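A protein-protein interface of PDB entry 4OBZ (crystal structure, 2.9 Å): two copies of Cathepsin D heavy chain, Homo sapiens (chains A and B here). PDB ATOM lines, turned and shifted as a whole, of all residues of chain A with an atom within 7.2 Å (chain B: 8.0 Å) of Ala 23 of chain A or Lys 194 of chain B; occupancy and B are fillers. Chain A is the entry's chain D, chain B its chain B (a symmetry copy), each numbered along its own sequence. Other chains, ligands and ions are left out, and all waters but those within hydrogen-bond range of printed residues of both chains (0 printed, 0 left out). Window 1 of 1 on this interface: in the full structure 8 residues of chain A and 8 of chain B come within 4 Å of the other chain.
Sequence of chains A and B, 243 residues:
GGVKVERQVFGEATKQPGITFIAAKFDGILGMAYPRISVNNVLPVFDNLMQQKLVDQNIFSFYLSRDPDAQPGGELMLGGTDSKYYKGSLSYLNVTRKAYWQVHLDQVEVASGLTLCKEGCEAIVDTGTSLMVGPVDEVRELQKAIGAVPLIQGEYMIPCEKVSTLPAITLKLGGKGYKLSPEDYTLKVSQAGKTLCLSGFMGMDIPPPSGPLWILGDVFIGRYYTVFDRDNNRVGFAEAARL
N of Val 189 of chain B sits at hydrogen-bond distance from O of Leu 196 of chain B (2.9 Å).
Hydrophobic or aromatic side chains of chain B within 4 Å of the printed part of chain A: Leu 196.
Along chain B the printed residues that touch a printed residue of chain A span positions 192 to 196.
Of the 9 printed residues of chain A, 4 touch a printed residue of chain B.
Hydrophobic or aromatic side chains of chain A that line the printed part of chain B: Ile 22.
Along chain A the printed residues that touch a printed residue of chain B span positions 22 to 25.
Among the printed residues, 7 pairs touch across the chains.
Among the printed residues, no Asp or Glu carboxylate lies within 4 Å of a Lys or Arg side-chain nitrogen of the other chain.
O of Ala 23 of chain A lies within hydrogen-bond range of NZ of Lys 194 of chain B, at 3.3 Å.
The backbone carbonyl oxygen of Ala 192 of chain B lies within hydrogen-bond range of the side-chain amino group of Lys 25 of chain A (2.9 Å).
Ile 22 of chain A touches Lys 194 of chain B.
Leu 196 of chain B touches Ile 22 of chain A (CD1 to CG2, 3.6 Å).
Lys 194 of chain B touches Ala 24 of chain A.
Lys 25 of chain A touches Gly 193 of chain B.
CE of Lys 194 of chain B touches CA of Lys 25 of chain A, at 3.8 Å.
No position is printed for both chains.
Ala 23 of chain A touches one residue of chain B.
Lys 194 of chain B touches just these residues of chain A: Ile 22, Ala 23, Ala 24 and Lys 25.
Ala 24 of chain A touches just one residue of chain B: Lys 194 (3.6 Å).
Printed residues of chain A within 4 Å of Leu 196 of chain B: Ile 22 (3.6 Å).
Printed residues of chain A within 4 Å of Gly 193 of chain B: Lys 25 (3.99 Å).
The nearest residue of chain A that does not touch Lys 194 of chain B is Phe 26 of chain A (5.8 Å).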
ATOM      1  N   ILE A  19      22.621  22.941   1.252  1.00  0.00           N
ATOM      2  CA  ILE A  19      21.463  22.069   1.043  1.00  0.00           C
ATOM      3  C   ILE A  19      20.693  21.951   2.342  1.00  0.00           C
ATOM      4  O   ILE A  19      19.542  21.512   2.347  1.00  0.00           O
ATOM      5  CB  ILE A  19      21.845  20.670   0.440  1.00  0.00           C
ATOM      6  CG1 ILE A  19      22.976  19.957   1.227  1.00  0.00           C
ATOM      7  CG2 ILE A  19      22.174  20.758  -1.034  1.00  0.00           C
ATOM      8  CD1 ILE A  19      22.498  18.864   2.206  1.00  0.00           C
ATOM      9  N   THR A  20      21.343  22.362   3.440  1.00  0.00           N
ATOM     10  CA  THR A  20      20.840  22.323   4.812  1.00  0.00           C
ATOM     11  C   THR A  20      19.399  22.790   4.906  1.00  0.00           C
ATOM     12  O   THR A  20      18.568  22.112   5.523  1.00  0.00           O
ATOM     13  CB  THR A  20      21.706  23.215   5.757  1.00  0.00           C
ATOM     14  OG1 THR A  20      22.886  23.697   5.097  1.00  0.00           O
ATOM     15  CG2 THR A  20      22.048  22.528   7.069  1.00  0.00           C
ATOM     16  N   PHE A  21      19.110  23.953   4.295  1.00  0.00           N
ATOM     17  CA  PHE A  21      17.809  24.576   4.414  1.00  0.00           C
ATOM     18  C   PHE A  21      16.844  24.153   3.342  1.00  0.00           C
ATOM     19  O   PHE A  21      15.641  24.324   3.533  1.00  0.00           O
ATOM     20  CB  PHE A  21      17.953  26.100   4.518  1.00  0.00           C
ATOM     21  CG  PHE A  21      18.649  26.493   5.807  1.00  0.00           C
ATOM     22  CD1 PHE A  21      18.054  26.248   7.044  1.00  0.00           C
ATOM     23  CD2 PHE A  21      19.908  27.082   5.785  1.00  0.00           C
ATOM     24  CE1 PHE A  21      18.703  26.597   8.228  1.00  0.00           C
ATOM     25  CE2 PHE A  21      20.551  27.435   6.972  1.00  0.00           C
ATOM     26  CZ  PHE A  21      19.947  27.193   8.184  1.00  0.00           C
ATOM     27  N   ILE A  22      17.332  23.548   2.251  1.00  0.00           N
ATOM     28  CA  ILE A  22      16.472  23.032   1.186  1.00  0.00           C
ATOM     29  C   ILE A  22      15.687  21.873   1.822  1.00  0.00           C
ATOM     30  O   ILE A  22      14.453  21.937   1.908  1.00  0.00           O
ATOM     31  CB  ILE A  22      17.306  22.585  -0.039  1.00  0.00           C
ATOM     32  CG1 ILE A  22      18.174  23.745  -0.551  1.00  0.00           C
ATOM     33  CG2 ILE A  22      16.380  22.058  -1.117  1.00  0.00           C
ATOM     34  CD1 ILE A  22      19.195  23.415  -1.548  1.00  0.00           C
ATOM     35  N   ALA A  23      16.451  20.890   2.369  1.00  0.00           N
ATOM     36  CA  ALA A  23      16.037  19.689   3.089  1.00  0.00           C
ATOM     37  C   ALA A  23      15.031  19.970   4.246  1.00  0.00           C
ATOM     38  O   ALA A  23      14.004  19.286   4.350  1.00  0.00           O
ATOM     39  CB  ALA A  23      17.278  18.992   3.637  1.00  0.00           C
ATOM     40  N   ALA A  24      15.333  20.992   5.085  1.00  0.00           N
ATOM     41  CA  ALA A  24      14.563  21.422   6.255  1.00  0.00           C
ATOM     42  C   ALA A  24      13.080  21.663   5.980  1.00  0.00           C
ATOM     43  O   ALA A  24      12.731  22.285   4.977  1.00  0.00           O
ATOM     44  CB  ALA A  24      15.198  22.660   6.856  1.00  0.00           C
ATOM     45  N   LYS A  25      12.215  21.153   6.882  1.00  0.00           N
ATOM     46  CA  LYS A  25      10.757  21.257   6.807  1.00  0.00           C
ATOM     47  C   LYS A  25      10.242  22.599   7.363  1.00  0.00           C
ATOM     48  O   LYS A  25       9.119  23.012   7.036  1.00  0.00           O
ATOM     49  CB  LYS A  25      10.103  20.074   7.539  1.00  0.00           C
ATOM     50  CG  LYS A  25       8.766  19.680   6.934  1.00  0.00           C
ATOM     51  CD  LYS A  25       8.429  18.209   7.163  1.00  0.00           C
ATOM     52  CE  LYS A  25       6.960  17.903   6.941  1.00  0.00           C
ATOM     53  NZ  LYS A  25       6.599  17.665   5.507  1.00  0.00           N
ATOM     54  N   PHE A  26      11.051  23.271   8.195  1.00  0.00           N
ATOM     55  CA  PHE A  26      10.701  24.547   8.796  1.00  0.00           C
ATOM     56  C   PHE A  26      11.142  25.698   7.897  1.00  0.00           C
ATOM     57  O   PHE A  26      12.030  25.508   7.080  1.00  0.00           O
ATOM     58  CB  PHE A  26      11.334  24.660  10.199  1.00  0.00           C
ATOM     59  CG  PHE A  26      12.802  24.331  10.247  1.00  0.00           C
ATOM     60  CD1 PHE A  26      13.762  25.312  10.007  1.00  0.00           C
ATOM     61  CD2 PHE A  26      13.230  23.038  10.505  1.00  0.00           C
ATOM     62  CE1 PHE A  26      15.130  24.999  10.025  1.00  0.00           C
ATOM     63  CE2 PHE A  26      14.596  22.730  10.546  1.00  0.00           C
ATOM     64  CZ  PHE A  26      15.536  23.713  10.299  1.00  0.00           C
ATOM     65  N   ASP A  27      10.548  26.882   8.054  1.00  0.00           N
ATOM     66  CA  ASP A  27      10.910  28.075   7.284  1.00  0.00           C
ATOM     67  C   ASP A  27      12.092  28.847   7.898  1.00  0.00           C
ATOM     68  O   ASP A  27      12.898  29.397   7.157  1.00  0.00           O
ATOM     69  CB  ASP A  27       9.701  29.020   7.077  1.00  0.00           C
ATOM     70  CG  ASP A  27       8.450  28.374   6.477  1.00  0.00           C
ATOM     71  OD1 ASP A  27       8.565  27.711   5.392  1.00  0.00           O
ATOM     72  OD2 ASP A  27       7.357  28.528   7.081  1.00  0.00           O
ATOM     73  N   LYS B 188      10.807  15.952 -11.447  1.00  0.00           N
ATOM     74  CA  LYS B 188       9.954  16.411 -10.345  1.00  0.00           C
ATOM     75  C   LYS B 188      10.289  15.604  -9.058  1.00  0.00           C
ATOM     76  O   LYS B 188       9.604  14.620  -8.723  1.00  0.00           O
ATOM     77  CB  LYS B 188       8.481  16.252 -10.734  1.00  0.00           C
ATOM     78  CG  LYS B 188       7.548  17.204 -10.006  1.00  0.00           C
ATOM     79  CD  LYS B 188       6.093  17.155 -10.520  1.00  0.00           C
ATOM     80  CE  LYS B 188       5.243  16.044  -9.929  1.00  0.00           C
ATOM     81  NZ  LYS B 188       4.868  16.307  -8.509  1.00  0.00           N
ATOM     82  N   VAL B 189      11.368  16.043  -8.349  1.00  0.00           N
ATOM     83  CA  VAL B 189      11.901  15.450  -7.112  1.00  0.00           C
ATOM     84  C   VAL B 189      11.115  15.934  -5.907  1.00  0.00           C
ATOM     85  O   VAL B 189      11.189  17.110  -5.570  1.00  0.00           O
ATOM     86  CB  VAL B 189      13.426  15.690  -6.939  1.00  0.00           C
ATOM     87  CG1 VAL B 189      13.884  15.342  -5.528  1.00  0.00           C
ATOM     88  CG2 VAL B 189      14.232  14.907  -7.971  1.00  0.00           C
ATOM     89  N   SER B 190      10.367  15.029  -5.262  1.00  0.00           N
ATOM     90  CA  SER B 190       9.581  15.368  -4.079  1.00  0.00           C
ATOM     91  C   SER B 190      10.229  14.760  -2.864  1.00  0.00           C
ATOM     92  O   SER B 190      10.820  13.687  -2.965  1.00  0.00           O
ATOM     93  CB  SER B 190       8.131  14.925  -4.227  1.00  0.00           C
ATOM     94  OG  SER B 190       7.528  15.561  -5.344  1.00  0.00           O
ATOM     95  N   GLN B 191      10.185  15.489  -1.734  1.00  0.00           N
ATOM     96  CA  GLN B 191      10.794  15.116  -0.448  1.00  0.00           C
ATOM     97  C   GLN B 191      10.215  15.960   0.677  1.00  0.00           C
ATOM     98  O   GLN B 191      10.074  17.178   0.523  1.00  0.00           O
ATOM     99  CB  GLN B 191      12.335  15.286  -0.479  1.00  0.00           C
ATOM    100  CG  GLN B 191      12.837  16.707  -0.847  1.00  0.00           C
ATOM    101  CD  GLN B 191      14.342  16.823  -0.882  1.00  0.00           C
ATOM    102  OE1 GLN B 191      14.942  17.059  -1.948  1.00  0.00           O
ATOM    103  NE2 GLN B 191      14.981  16.661   0.285  1.00  0.00           N
ATOM    104  N   ALA B 192       9.905  15.309   1.814  1.00  0.00           N
ATOM    105  CA  ALA B 192       9.342  15.927   3.017  1.00  0.00           C
ATOM    106  C   ALA B 192       8.215  16.900   2.664  1.00  0.00           C
ATOM    107  O   ALA B 192       8.194  18.038   3.150  1.00  0.00           O
ATOM    108  CB  ALA B 192      10.441  16.629   3.819  1.00  0.00           C
ATOM    109  N   GLY B 193       7.331  16.464   1.769  1.00  0.00           N
ATOM    110  CA  GLY B 193       6.187  17.256   1.320  1.00  0.00           C
ATOM    111  C   GLY B 193       6.497  18.554   0.595  1.00  0.00           C
ATOM    112  O   GLY B 193       5.730  19.522   0.671  1.00  0.00           O
ATOM    113  N   LYS B 194       7.614  18.571  -0.125  1.00  0.00           N
ATOM    114  CA  LYS B 194       8.065  19.708  -0.908  1.00  0.00           C
ATOM    115  C   LYS B 194       8.533  19.178  -2.257  1.00  0.00           C
ATOM    116  O   LYS B 194       9.141  18.104  -2.314  1.00  0.00           O
ATOM    117  CB  LYS B 194       9.185  20.467  -0.168  1.00  0.00           C
ATOM    118  CG  LYS B 194       8.692  21.294   1.048  1.00  0.00           C
ATOM    119  CD  LYS B 194       9.815  21.723   2.020  1.00  0.00           C
ATOM    120  CE  LYS B 194      10.200  20.670   3.052  1.00  0.00           C
ATOM    121  NZ  LYS B 194      11.295  19.758   2.591  1.00  0.00           N
ATOM    122  N   THR B 195       8.207  19.919  -3.348  1.00  0.00           N
ATOM    123  CA  THR B 195       8.551  19.563  -4.734  1.00  0.00           C
ATOM    124  C   THR B 195       9.569  20.524  -5.373  1.00  0.00           C
ATOM    125  O   THR B 195       9.377  21.741  -5.392  1.00  0.00           O
ATOM    126  CB  THR B 195       7.263  19.429  -5.584  1.00  0.00           C
ATOM    127  OG1 THR B 195       6.446  18.403  -5.030  1.00  0.00           O
ATOM    128  CG2 THR B 195       7.539  19.102  -7.045  1.00  0.00           C
ATOM    129  N   LEU B 196      10.631  19.953  -5.921  1.00  0.00           N
ATOM    130  CA  LEU B 196      11.663  20.665  -6.664  1.00  0.00           C
ATOM    131  C   LEU B 196      11.820  20.068  -8.065  1.00  0.00           C
ATOM    132  O   LEU B 196      11.491  18.900  -8.300  1.00  0.00           O
ATOM    133  CB  LEU B 196      13.000  20.637  -5.927  1.00  0.00           C
ATOM    134  CG  LEU B 196      13.221  21.691  -4.826  1.00  0.00           C
ATOM    135  CD1 LEU B 196      14.546  21.475  -4.147  1.00  0.00           C
ATOM    136  CD2 LEU B 196      13.176  23.100  -5.369  1.00  0.00           C
ATOM    137  N   CYS B 197      12.303  20.881  -9.004  1.00  0.00           N
ATOM    138  CA  CYS B 197      12.496  20.413 -10.369  1.00  0.00           C
ATOM    139  C   CYS B 197      13.979  20.377 -10.735  1.00  0.00           C
ATOM    140  O   CYS B 197      14.651  21.393 -10.881  1.00  0.00           O
ATOM    141  CB  CYS B 197      11.641  21.199 -11.360  1.00  0.00           C
ATOM    142  SG  CYS B 197       9.846  21.007 -11.097  1.00  0.00           S
